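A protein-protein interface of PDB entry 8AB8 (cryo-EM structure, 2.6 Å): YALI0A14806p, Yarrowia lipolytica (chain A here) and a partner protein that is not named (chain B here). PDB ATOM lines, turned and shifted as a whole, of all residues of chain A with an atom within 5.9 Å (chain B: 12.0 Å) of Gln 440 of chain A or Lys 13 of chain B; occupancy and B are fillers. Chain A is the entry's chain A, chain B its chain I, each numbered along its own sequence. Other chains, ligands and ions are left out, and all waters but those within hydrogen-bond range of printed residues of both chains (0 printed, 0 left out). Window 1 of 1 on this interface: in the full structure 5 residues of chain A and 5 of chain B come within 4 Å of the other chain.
The side-chain hydroxyl (OG) of Ser 16 of chain B lies within hydrogen-bond range of the backbone carbonyl oxygen (O) of Trp 474 of chain A (2.9 Å).
The backbone carbonyl oxygen (O) of Trp 474 of chain A sits close to the backbone NH (N) of Asn 15 of chain B (3.4 Å).
The side-chain amino group (NZ) of Lys 13 of chain B is in hydrogen-bond range of the side-chain amide oxygen (OE1) of Gln 440 of chain A (3.1 Å).
The backbone NH (N) of Tyr 444 of chain A is in hydrogen-bond range of the backbone carbonyl oxygen (O) of Ala 439 of chain A (2.9 Å).
The side-chain amino group of Lys 13 of chain B sits at hydrogen-bond distance from the side-chain amide oxygen of Asn 9 of chain B (3.2 Å).
The backbone carbonyl oxygen (O) of Asn 9 of chain B is in hydrogen-bond range of the guanidinium group (NH1) of Arg 14 of chain B, 3.2 Å away.
N of Lys 13 of chain B sits at hydrogen-bond distance from O of Tyr 8 of chain B (2.8 Å).
The side-chain amide nitrogen (NE2) of Gln 440 of chain A lies within hydrogen-bond range of the backbone carbonyl oxygen (O) of Ser 374 of chain A, at 2.8 Å.
Among the printed residues, pairs that only touch across the chains: Tyr 444 of chain A with Lys 13 of chain B, Trp 474 of chain A with Lys 13 of chain B and Trp 474 of chain A with Arg 14 of chain B.
No residue of chain B comes within 4 Å of Ser 374 of chain A.
No residue of chain B comes within 4 Å of Thr 375 of chain A.
No residue of chain B comes within 4 Å of Arg 436 of chain A.
No residue of chain B comes within 4 Å of Ala 439 of chain A.
Of the printed residues of chain B, Gln 440 of chain A touches Lys 13.
No residue of chain B comes within 4 Å of Thr 442 of chain A.
No residue of chain B comes within 4 Å of Leu 443 of chain A.
Tyr 444 of chain A touches just one residue of chain B: Lys 13.
Trp 474 of chain A touches four residues of chain B.
Ala 4 of chain B touches none of the printed residues of chain A.
Of chain A, only Gln 440, Tyr 444 and Trp 474 come within 4 Å of Lys 13 of chain B.
Of the printed residues of chain A, Arg 14 of chain B touches Trp 474.
Of the printed residues of chain A, Asn 15 of chain B touches Trp 474 (3.3 Å).
Of the printed residues of chain A, Ser 16 of chain B touches Trp 474.
Ile 22 of chain B touches none of the printed residues of chain A.
The nearest printed residue of chain B that does not touch Gln 440 of chain A is Arg 14 of chain B (4.01 Å).
The nearest printed residue of chain A that does not touch Lys 13 of chain B is Lys 441 of chain A (5.9 Å).
The nearest printed residue of chain A that does not touch Arg 14 of chain B is Gln 440 of chain A (4.01 Å).
Among the printed residues, no Asp or Glu carboxylate lies within 4 Å of a Lys or Arg side-chain nitrogen of the other chain.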
ATOM      1  N   LEU A 373      20.651   8.837  -1.678  1.00  0.00           N
ATOM      2  CA  LEU A 373      20.999   9.620  -2.856  1.00  0.00           C
ATOM      3  C   LEU A 373      22.425  10.139  -2.715  1.00  0.00           C
ATOM      4  O   LEU A 373      23.079  10.389  -3.715  1.00  0.00           O
ATOM      5  CB  LEU A 373      20.029  10.787  -3.056  1.00  0.00           C
ATOM      6  CG  LEU A 373      18.589  10.420  -3.411  1.00  0.00           C
ATOM      7  CD1 LEU A 373      17.699  11.652  -3.409  1.00  0.00           C
ATOM      8  CD2 LEU A 373      18.522   9.735  -4.758  1.00  0.00           C
ATOM      9  N   SER A 374      22.888  10.307  -1.469  1.00  0.00           N
ATOM     10  CA  SER A 374      24.228  10.789  -1.173  1.00  0.00           C
ATOM     11  C   SER A 374      25.202   9.618  -1.068  1.00  0.00           C
ATOM     12  O   SER A 374      26.360   9.754  -1.445  1.00  0.00           O
ATOM     13  CB  SER A 374      24.269  11.601   0.109  1.00  0.00           C
ATOM     14  OG  SER A 374      23.491  12.790   0.030  1.00  0.00           O
ATOM     15  N   THR A 375      24.759   8.480  -0.528  1.00  0.00           N
ATOM     16  CA  THR A 375      25.729   7.475  -0.125  1.00  0.00           C
ATOM     17  C   THR A 375      25.797   6.295  -1.091  1.00  0.00           C
ATOM     18  O   THR A 375      26.852   5.680  -1.209  1.00  0.00           O
ATOM     19  CB  THR A 375      25.431   6.935   1.275  1.00  0.00           C
ATOM     20  OG1 THR A 375      24.234   6.170   1.136  1.00  0.00           O
ATOM     21  CG2 THR A 375      25.244   8.020   2.312  1.00  0.00           C
ATOM     22  N   VAL A 435      24.379  13.062  -9.415  1.00  0.00           N
ATOM     23  CA  VAL A 435      23.318  12.897  -8.441  1.00  0.00           C
ATOM     24  C   VAL A 435      23.918  12.878  -7.036  1.00  0.00           C
ATOM     25  O   VAL A 435      23.445  13.613  -6.168  1.00  0.00           O
ATOM     26  CB  VAL A 435      22.445  11.668  -8.756  1.00  0.00           C
ATOM     27  CG1 VAL A 435      21.414  11.405  -7.669  1.00  0.00           C
ATOM     28  CG2 VAL A 435      21.752  11.843 -10.098  1.00  0.00           C
ATOM     29  N   ARG A 436      24.988  12.090  -6.836  1.00  0.00           N
ATOM     30  CA  ARG A 436      25.635  12.024  -5.531  1.00  0.00           C
ATOM     31  C   ARG A 436      26.161  13.399  -5.120  1.00  0.00           C
ATOM     32  O   ARG A 436      25.968  13.825  -3.983  1.00  0.00           O
ATOM     33  CB  ARG A 436      26.761  10.990  -5.473  1.00  0.00           C
ATOM     34  CG  ARG A 436      26.302   9.539  -5.505  1.00  0.00           C
ATOM     35  CD  ARG A 436      27.444   8.628  -5.948  1.00  0.00           C
ATOM     36  NE  ARG A 436      28.362   8.557  -4.826  1.00  0.00           N
ATOM     37  CZ  ARG A 436      28.167   7.787  -3.760  1.00  0.00           C
ATOM     38  NH1 ARG A 436      27.119   6.978  -3.700  1.00  0.00           N
ATOM     39  NH2 ARG A 436      29.030   7.814  -2.761  1.00  0.00           N
ATOM     40  N   ALA A 437      26.803  14.106  -6.048  1.00  0.00           N
ATOM     41  CA  ALA A 437      27.364  15.399  -5.698  1.00  0.00           C
ATOM     42  C   ALA A 437      26.255  16.374  -5.309  1.00  0.00           C
ATOM     43  O   ALA A 437      26.425  17.161  -4.376  1.00  0.00           O
ATOM     44  CB  ALA A 437      28.189  15.931  -6.833  1.00  0.00           C
ATOM     45  N   TRP A 438      25.135  16.315  -6.041  1.00  0.00           N
ATOM     46  CA  TRP A 438      24.021  17.213  -5.802  1.00  0.00           C
ATOM     47  C   TRP A 438      23.415  16.920  -4.435  1.00  0.00           C
ATOM     48  O   TRP A 438      23.153  17.852  -3.672  1.00  0.00           O
ATOM     49  CB  TRP A 438      22.989  17.135  -6.933  1.00  0.00           C
ATOM     50  CG  TRP A 438      21.777  17.971  -6.671  1.00  0.00           C
ATOM     51  CD1 TRP A 438      21.613  19.303  -6.925  1.00  0.00           C
ATOM     52  CD2 TRP A 438      20.561  17.519  -6.058  1.00  0.00           C
ATOM     53  NE1 TRP A 438      20.373  19.711  -6.508  1.00  0.00           N
ATOM     54  CE2 TRP A 438      19.698  18.637  -5.988  1.00  0.00           C
ATOM     55  CE3 TRP A 438      20.125  16.283  -5.559  1.00  0.00           C
ATOM     56  CZ2 TRP A 438      18.426  18.556  -5.421  1.00  0.00           C
ATOM     57  CZ3 TRP A 438      18.863  16.201  -5.013  1.00  0.00           C
ATOM     58  CH2 TRP A 438      18.032  17.325  -4.943  1.00  0.00           C
ATOM     59  N   ALA A 439      23.201  15.632  -4.133  1.00  0.00           N
ATOM     60  CA  ALA A 439      22.521  15.274  -2.899  1.00  0.00           C
ATOM     61  C   ALA A 439      23.394  15.620  -1.695  1.00  0.00           C
ATOM     62  O   ALA A 439      22.881  16.034  -0.653  1.00  0.00           O
ATOM     63  CB  ALA A 439      22.119  13.828  -2.920  1.00  0.00           C
ATOM     64  N   GLN A 440      24.717  15.518  -1.877  1.00  0.00           N
ATOM     65  CA  GLN A 440      25.638  15.758  -0.780  1.00  0.00           C
ATOM     66  C   GLN A 440      25.702  17.238  -0.425  1.00  0.00           C
ATOM     67  O   GLN A 440      26.006  17.574   0.718  1.00  0.00           O
ATOM     68  CB  GLN A 440      27.010  15.186  -1.081  1.00  0.00           C
ATOM     69  CG  GLN A 440      27.039  13.691  -0.858  1.00  0.00           C
ATOM     70  CD  GLN A 440      28.323  13.093  -1.369  1.00  0.00           C
ATOM     71  OE1 GLN A 440      29.317  13.782  -1.583  1.00  0.00           O
ATOM     72  NE2 GLN A 440      28.302  11.793  -1.602  1.00  0.00           N
ATOM     73  N   LYS A 441      25.371  18.111  -1.375  1.00  0.00           N
ATOM     74  CA  LYS A 441      25.380  19.528  -1.056  1.00  0.00           C
ATOM     75  C   LYS A 441      23.980  20.073  -0.781  1.00  0.00           C
ATOM     76  O   LYS A 441      23.867  21.159  -0.222  1.00  0.00           O
ATOM     77  CB  LYS A 441      26.139  20.337  -2.103  1.00  0.00           C
ATOM     78  CG  LYS A 441      25.434  20.487  -3.427  1.00  0.00           C
ATOM     79  CD  LYS A 441      26.163  21.524  -4.239  1.00  0.00           C
ATOM     80  CE  LYS A 441      25.304  22.117  -5.329  1.00  0.00           C
ATOM     81  NZ  LYS A 441      25.772  21.739  -6.688  1.00  0.00           N
ATOM     82  N   THR A 442      22.931  19.336  -1.161  1.00  0.00           N
ATOM     83  CA  THR A 442      21.571  19.857  -1.099  1.00  0.00           C
ATOM     84  C   THR A 442      20.747  19.170  -0.015  1.00  0.00           C
ATOM     85  O   THR A 442      19.881  19.791   0.592  1.00  0.00           O
ATOM     86  CB  THR A 442      20.887  19.704  -2.462  1.00  0.00           C
ATOM     87  OG1 THR A 442      21.764  20.321  -3.402  1.00  0.00           O
ATOM     88  CG2 THR A 442      19.522  20.348  -2.544  1.00  0.00           C
ATOM     89  N   LEU A 443      20.982  17.876   0.188  1.00  0.00           N
ATOM     90  CA  LEU A 443      20.128  17.103   1.065  1.00  0.00           C
ATOM     91  C   LEU A 443      20.879  16.700   2.317  1.00  0.00           C
ATOM     92  O   LEU A 443      20.318  16.713   3.410  1.00  0.00           O
ATOM     93  CB  LEU A 443      19.705  15.837   0.326  1.00  0.00           C
ATOM     94  CG  LEU A 443      18.490  15.985  -0.572  1.00  0.00           C
ATOM     95  CD1 LEU A 443      18.348  14.724  -1.399  1.00  0.00           C
ATOM     96  CD2 LEU A 443      17.244  16.201   0.280  1.00  0.00           C
ATOM     97  N   TYR A 444      22.126  16.268   2.133  1.00  0.00           N
ATOM     98  CA  TYR A 444      22.788  15.563   3.210  1.00  0.00           C
ATOM     99  C   TYR A 444      23.012  16.497   4.395  1.00  0.00           C
ATOM    100  O   TYR A 444      23.613  17.552   4.210  1.00  0.00           O
ATOM    101  CB  TYR A 444      24.111  14.973   2.741  1.00  0.00           C
ATOM    102  CG  TYR A 444      24.536  13.895   3.690  1.00  0.00           C
ATOM    103  CD1 TYR A 444      23.920  12.656   3.636  1.00  0.00           C
ATOM    104  CD2 TYR A 444      25.481  14.126   4.677  1.00  0.00           C
ATOM    105  CE1 TYR A 444      24.252  11.647   4.521  1.00  0.00           C
ATOM    106  CE2 TYR A 444      25.821  13.128   5.577  1.00  0.00           C
ATOM    107  CZ  TYR A 444      25.204  11.889   5.497  1.00  0.00           C
ATOM    108  OH  TYR A 444      25.536  10.902   6.379  1.00  0.00           O
ATOM    109  N   LYS A 446      21.103  18.564   5.978  1.00  0.00           N
ATOM    110  CA  LYS A 446      20.629  19.918   5.736  1.00  0.00           C
ATOM    111  C   LYS A 446      19.371  20.167   6.553  1.00  0.00           C
ATOM    112  O   LYS A 446      18.729  19.226   6.994  1.00  0.00           O
ATOM    113  CB  LYS A 446      20.352  20.137   4.249  1.00  0.00           C
ATOM    114  CG  LYS A 446      21.588  20.206   3.371  1.00  0.00           C
ATOM    115  CD  LYS A 446      22.435  21.442   3.606  1.00  0.00           C
ATOM    116  CE  LYS A 446      22.177  22.535   2.593  1.00  0.00           C
ATOM    117  NZ  LYS A 446      22.728  23.840   3.035  1.00  0.00           N
ATOM    118  N   TRP A 474      27.773   6.302   7.772  1.00  0.00           N
ATOM    119  CA  TRP A 474      28.488   6.801   6.609  1.00  0.00           C
ATOM    120  C   TRP A 474      29.459   7.902   7.035  1.00  0.00           C
ATOM    121  O   TRP A 474      30.664   7.617   6.944  1.00  0.00           O
ATOM    122  CB  TRP A 474      27.515   7.307   5.545  1.00  0.00           C
ATOM    123  CG  TRP A 474      28.123   7.662   4.220  1.00  0.00           C
ATOM    124  CD1 TRP A 474      28.568   6.800   3.257  1.00  0.00           C
ATOM    125  CD2 TRP A 474      28.271   8.986   3.670  1.00  0.00           C
ATOM    126  NE1 TRP A 474      29.004   7.498   2.163  1.00  0.00           N
ATOM    127  CE2 TRP A 474      28.840   8.840   2.384  1.00  0.00           C
ATOM    128  CE3 TRP A 474      27.975  10.275   4.134  1.00  0.00           C
ATOM    129  CZ2 TRP A 474      29.117   9.938   1.563  1.00  0.00           C
ATOM    130  CZ3 TRP A 474      28.246  11.364   3.326  1.00  0.00           C
ATOM    131  CH2 TRP A 474      28.815  11.193   2.055  1.00  0.00           C
ATOM    132  N   ALA B   4      35.894  26.461   4.194  1.00  0.00           N
ATOM    133  CA  ALA B   4      34.796  26.011   5.152  1.00  0.00           C
ATOM    134  C   ALA B   4      33.959  24.905   4.523  1.00  0.00           C
ATOM    135  O   ALA B   4      33.699  23.883   5.161  1.00  0.00           O
ATOM    136  CB  ALA B   4      33.920  27.164   5.581  1.00  0.00           C
ATOM    137  N   THR B   5      33.540  25.124   3.277  1.00  0.00           N
ATOM    138  CA  THR B   5      32.947  24.044   2.517  1.00  0.00           C
ATOM    139  C   THR B   5      33.935  22.886   2.409  1.00  0.00           C
ATOM    140  O   THR B   5      33.557  21.731   2.621  1.00  0.00           O
ATOM    141  CB  THR B   5      32.503  24.542   1.145  1.00  0.00           C
ATOM    142  OG1 THR B   5      31.553  25.566   1.438  1.00  0.00           O
ATOM    143  CG2 THR B   5      31.889  23.444   0.305  1.00  0.00           C
ATOM    144  N   THR B   6      35.182  23.218   2.059  1.00  0.00           N
ATOM    145  CA  THR B   6      36.213  22.214   1.883  1.00  0.00           C
ATOM    146  C   THR B   6      36.413  21.469   3.191  1.00  0.00           C
ATOM    147  O   THR B   6      36.367  20.245   3.215  1.00  0.00           O
ATOM    148  CB  THR B   6      37.528  22.844   1.436  1.00  0.00           C
ATOM    149  OG1 THR B   6      37.224  23.404   0.161  1.00  0.00           O
ATOM    150  CG2 THR B   6      38.632  21.818   1.331  1.00  0.00           C
ATOM    151  N   PHE B   7      36.596  22.228   4.271  1.00  0.00           N
ATOM    152  CA  PHE B   7      36.810  21.620   5.567  1.00  0.00           C
ATOM    153  C   PHE B   7      35.633  20.722   5.941  1.00  0.00           C
ATOM    154  O   PHE B   7      35.853  19.602   6.391  1.00  0.00           O
ATOM    155  CB  PHE B   7      37.114  22.669   6.631  1.00  0.00           C
ATOM    156  CG  PHE B   7      37.748  22.076   7.859  1.00  0.00           C
ATOM    157  CD1 PHE B   7      36.964  21.544   8.877  1.00  0.00           C
ATOM    158  CD2 PHE B   7      39.130  22.022   7.988  1.00  0.00           C
ATOM    159  CE1 PHE B   7      37.546  20.995  10.013  1.00  0.00           C
ATOM    160  CE2 PHE B   7      39.711  21.465   9.121  1.00  0.00           C
ATOM    161  CZ  PHE B   7      38.919  20.950  10.129  1.00  0.00           C
ATOM    162  N   TYR B   8      34.401  21.212   5.744  1.00  0.00           N
ATOM    163  CA  TYR B   8      33.219  20.431   6.069  1.00  0.00           C
ATOM    164  C   TYR B   8      33.218  19.124   5.278  1.00  0.00           C
ATOM    165  O   TYR B   8      33.012  18.052   5.849  1.00  0.00           O
ATOM    166  CB  TYR B   8      31.931  21.218   5.820  1.00  0.00           C
ATOM    167  CG  TYR B   8      30.701  20.374   6.021  1.00  0.00           C
ATOM    168  CD1 TYR B   8      30.194  20.147   7.296  1.00  0.00           C
ATOM    169  CD2 TYR B   8      30.088  19.742   4.948  1.00  0.00           C
ATOM    170  CE1 TYR B   8      29.096  19.326   7.502  1.00  0.00           C
ATOM    171  CE2 TYR B   8      28.988  18.920   5.137  1.00  0.00           C
ATOM    172  CZ  TYR B   8      28.488  18.716   6.415  1.00  0.00           C
ATOM    173  OH  TYR B   8      27.398  17.913   6.596  1.00  0.00           O
ATOM    174  N   ASN B   9      33.478  19.230   3.970  1.00  0.00           N
ATOM    175  CA  ASN B   9      33.387  18.107   3.053  1.00  0.00           C
ATOM    176  C   ASN B   9      34.415  17.027   3.361  1.00  0.00           C
ATOM    177  O   ASN B   9      34.131  15.843   3.191  1.00  0.00           O
ATOM    178  CB  ASN B   9      33.493  18.559   1.602  1.00  0.00           C
ATOM    179  CG  ASN B   9      32.175  19.131   1.141  1.00  0.00           C
ATOM    180  OD1 ASN B   9      31.121  18.726   1.625  1.00  0.00           O
ATOM    181  ND2 ASN B   9      32.226  20.080   0.226  1.00  0.00           N
ATOM    182  N   VAL B  10      35.596  17.439   3.830  1.00  0.00           N
ATOM    183  CA  VAL B  10      36.664  16.497   4.099  1.00  0.00           C
ATOM    184  C   VAL B  10      36.508  15.896   5.495  1.00  0.00           C
ATOM    185  O   VAL B  10      36.546  14.681   5.637  1.00  0.00           O
ATOM    186  CB  VAL B  10      38.048  17.126   3.860  1.00  0.00           C
ATOM    187  CG1 VAL B  10      39.168  16.183   4.260  1.00  0.00           C
ATOM    188  CG2 VAL B  10      38.204  17.537   2.407  1.00  0.00           C
ATOM    189  N   PHE B  11      36.297  16.722   6.518  1.00  0.00           N
ATOM    190  CA  PHE B  11      36.433  16.191   7.866  1.00  0.00           C
ATOM    191  C   PHE B  11      35.109  15.935   8.571  1.00  0.00           C
ATOM    192  O   PHE B  11      35.094  15.249   9.589  1.00  0.00           O
ATOM    193  CB  PHE B  11      37.278  17.123   8.724  1.00  0.00           C
ATOM    194  CG  PHE B  11      38.682  17.239   8.206  1.00  0.00           C
ATOM    195  CD1 PHE B  11      39.598  16.214   8.401  1.00  0.00           C
ATOM    196  CD2 PHE B  11      39.072  18.351   7.467  1.00  0.00           C
ATOM    197  CE1 PHE B  11      40.888  16.311   7.894  1.00  0.00           C
ATOM    198  CE2 PHE B  11      40.362  18.447   6.963  1.00  0.00           C
ATOM    199  CZ  PHE B  11      41.267  17.427   7.178  1.00  0.00           C
ATOM    200  N   VAL B  12      34.010  16.494   8.068  1.00  0.00           N
ATOM    201  CA  VAL B  12      32.814  16.515   8.893  1.00  0.00           C
ATOM    202  C   VAL B  12      31.678  15.736   8.242  1.00  0.00           C
ATOM    203  O   VAL B  12      30.993  14.976   8.924  1.00  0.00           O
ATOM    204  CB  VAL B  12      32.413  17.951   9.282  1.00  0.00           C
ATOM    205  CG1 VAL B  12      31.183  17.959  10.177  1.00  0.00           C
ATOM    206  CG2 VAL B  12      33.560  18.663   9.989  1.00  0.00           C
ATOM    207  N   LYS B  13      31.498  15.913   6.929  1.00  0.00           N
ATOM    208  CA  LYS B  13      30.354  15.369   6.214  1.00  0.00           C
ATOM    209  C   LYS B  13      30.198  13.865   6.452  1.00  0.00           C
ATOM    210  O   LYS B  13      29.117  13.413   6.807  1.00  0.00           O
ATOM    211  CB  LYS B  13      30.466  15.696   4.727  1.00  0.00           C
ATOM    212  CG  LYS B  13      29.393  15.077   3.838  1.00  0.00           C
ATOM    213  CD  LYS B  13      29.384  15.631   2.418  1.00  0.00           C
ATOM    214  CE  LYS B  13      30.608  15.248   1.610  1.00  0.00           C
ATOM    215  NZ  LYS B  13      30.609  15.888   0.273  1.00  0.00           N
ATOM    216  N   ARG B  14      31.248  13.078   6.209  1.00  0.00           N
ATOM    217  CA  ARG B  14      31.148  11.650   6.449  1.00  0.00           C
ATOM    218  C   ARG B  14      31.426  11.392   7.920  1.00  0.00           C
ATOM    219  O   ARG B  14      32.404  11.905   8.446  1.00  0.00           O
ATOM    220  CB  ARG B  14      32.171  10.896   5.603  1.00  0.00           C
ATOM    221  CG  ARG B  14      31.851  10.871   4.121  1.00  0.00           C
ATOM    222  CD  ARG B  14      33.087  10.510   3.325  1.00  0.00           C
ATOM    223  NE  ARG B  14      32.764  10.748   1.929  1.00  0.00           N
ATOM    224  CZ  ARG B  14      32.889  11.918   1.313  1.00  0.00           C
ATOM    225  NH1 ARG B  14      33.364  12.968   1.961  1.00  0.00           N
ATOM    226  NH2 ARG B  14      32.541  12.033   0.044  1.00  0.00           N
ATOM    227  N   ASN B  15      30.570  10.605   8.575  1.00  0.00           N
ATOM    228  CA  ASN B  15      30.742  10.355   9.992  1.00  0.00           C
ATOM    229  C   ASN B  15      32.000   9.527  10.228  1.00  0.00           C
ATOM    230  O   ASN B  15      32.703   9.717  11.218  1.00  0.00           O
ATOM    231  CB  ASN B  15      29.519   9.691  10.615  1.00  0.00           C
ATOM    232  CG  ASN B  15      29.529   9.819  12.120  1.00  0.00           C
ATOM    233  OD1 ASN B  15      29.776  10.905  12.647  1.00  0.00           O
ATOM    234  ND2 ASN B  15      29.266   8.727  12.820  1.00  0.00           N
ATOM    235  N   SER B  16      32.304   8.633   9.290  1.00  0.00           N
ATOM    236  CA  SER B  16      33.533   7.870   9.389  1.00  0.00           C
ATOM    237  C   SER B  16      34.724   8.821   9.463  1.00  0.00           C
ATOM    238  O   SER B  16      35.630   8.590  10.254  1.00  0.00           O
ATOM    239  CB  SER B  16      33.668   6.906   8.254  1.00  0.00           C
ATOM    240  OG  SER B  16      33.570   7.589   7.014  1.00  0.00           O
ATOM    241  N   ALA B  17      34.706   9.895   8.663  1.00  0.00           N
ATOM    242  CA  ALA B  17      35.810  10.843   8.658  1.00  0.00           C
ATOM    243  C   ALA B  17      35.806  11.688   9.930  1.00  0.00           C
ATOM    244  O   ALA B  17      36.866  12.057  10.432  1.00  0.00           O
ATOM    245  CB  ALA B  17      35.752  11.713   7.431  1.00  0.00           C
ATOM    246  N   PHE B  18      34.604  12.048  10.391  1.00  0.00           N
ATOM    247  CA  PHE B  18      34.425  12.884  11.562  1.00  0.00           C
ATOM    248  C   PHE B  18      34.930  12.138  12.791  1.00  0.00           C
ATOM    249  O   PHE B  18      35.633  12.725  13.606  1.00  0.00           O
ATOM    250  CB  PHE B  18      32.951  13.268  11.694  1.00  0.00           C
ATOM    251  CG  PHE B  18      32.602  14.315  12.723  1.00  0.00           C
ATOM    252  CD1 PHE B  18      33.277  15.528  12.766  1.00  0.00           C
ATOM    253  CD2 PHE B  18      31.546  14.112  13.604  1.00  0.00           C
ATOM    254  CE1 PHE B  18      32.924  16.508  13.683  1.00  0.00           C
ATOM    255  CE2 PHE B  18      31.194  15.095  14.522  1.00  0.00           C
ATOM    256  CZ  PHE B  18      31.885  16.290  14.560  1.00  0.00           C
ATOM    257  N   VAL B  19      34.585  10.845  12.896  1.00  0.00           N
ATOM    258  CA  VAL B  19      34.993  10.074  14.056  1.00  0.00           C
ATOM    259  C   VAL B  19      36.503   9.849  14.002  1.00  0.00           C
ATOM    260  O   VAL B  19      37.162   9.971  15.029  1.00  0.00           O
ATOM    261  CB  VAL B  19      34.199   8.765  14.210  1.00  0.00           C
ATOM    262  CG1 VAL B  19      34.885   7.779  15.151  1.00  0.00           C
ATOM    263  CG2 VAL B  19      32.768   9.033  14.656  1.00  0.00           C
ATOM    264  N   ALA B  20      37.047   9.564  12.807  1.00  0.00           N
ATOM    265  CA  ALA B  20      38.487   9.442  12.623  1.00  0.00           C
ATOM    266  C   ALA B  20      39.216  10.726  13.030  1.00  0.00           C
ATOM    267  O   ALA B  20      40.238  10.648  13.706  1.00  0.00           O
ATOM    268  CB  ALA B  20      38.844   9.017  11.218  1.00  0.00           C
ATOM    269  N   THR B  21      38.683  11.892  12.643  1.00  0.00           N
ATOM    270  CA  THR B  21      39.285  13.172  12.992  1.00  0.00           C
ATOM    271  C   THR B  21      39.245  13.412  14.500  1.00  0.00           C
ATOM    272  O   THR B  21      40.197  13.956  15.053  1.00  0.00           O
ATOM    273  CB  THR B  21      38.592  14.326  12.256  1.00  0.00           C
ATOM    274  OG1 THR B  21      38.629  14.008  10.867  1.00  0.00           O
ATOM    275  CG2 THR B  21      39.254  15.666  12.483  1.00  0.00           C
ATOM    276  N   ILE B  22      38.121  13.066  15.144  1.00  0.00           N
ATOM    277  CA  ILE B  22      37.943  13.266  16.576  1.00  0.00           C
ATOM    278  C   ILE B  22      38.956  12.399  17.332  1.00  0.00           C
ATOM    279  O   ILE B  22      39.621  12.896  18.234  1.00  0.00           O
ATOM    280  CB  ILE B  22      36.470  13.036  17.004  1.00  0.00           C
ATOM    281  CG1 ILE B  22      35.559  14.190  16.571  1.00  0.00           C
ATOM    282  CG2 ILE B  22      36.334  12.758  18.498  1.00  0.00           C
ATOM    283  CD1 ILE B  22      34.087  13.817  16.446  1.00  0.00           C
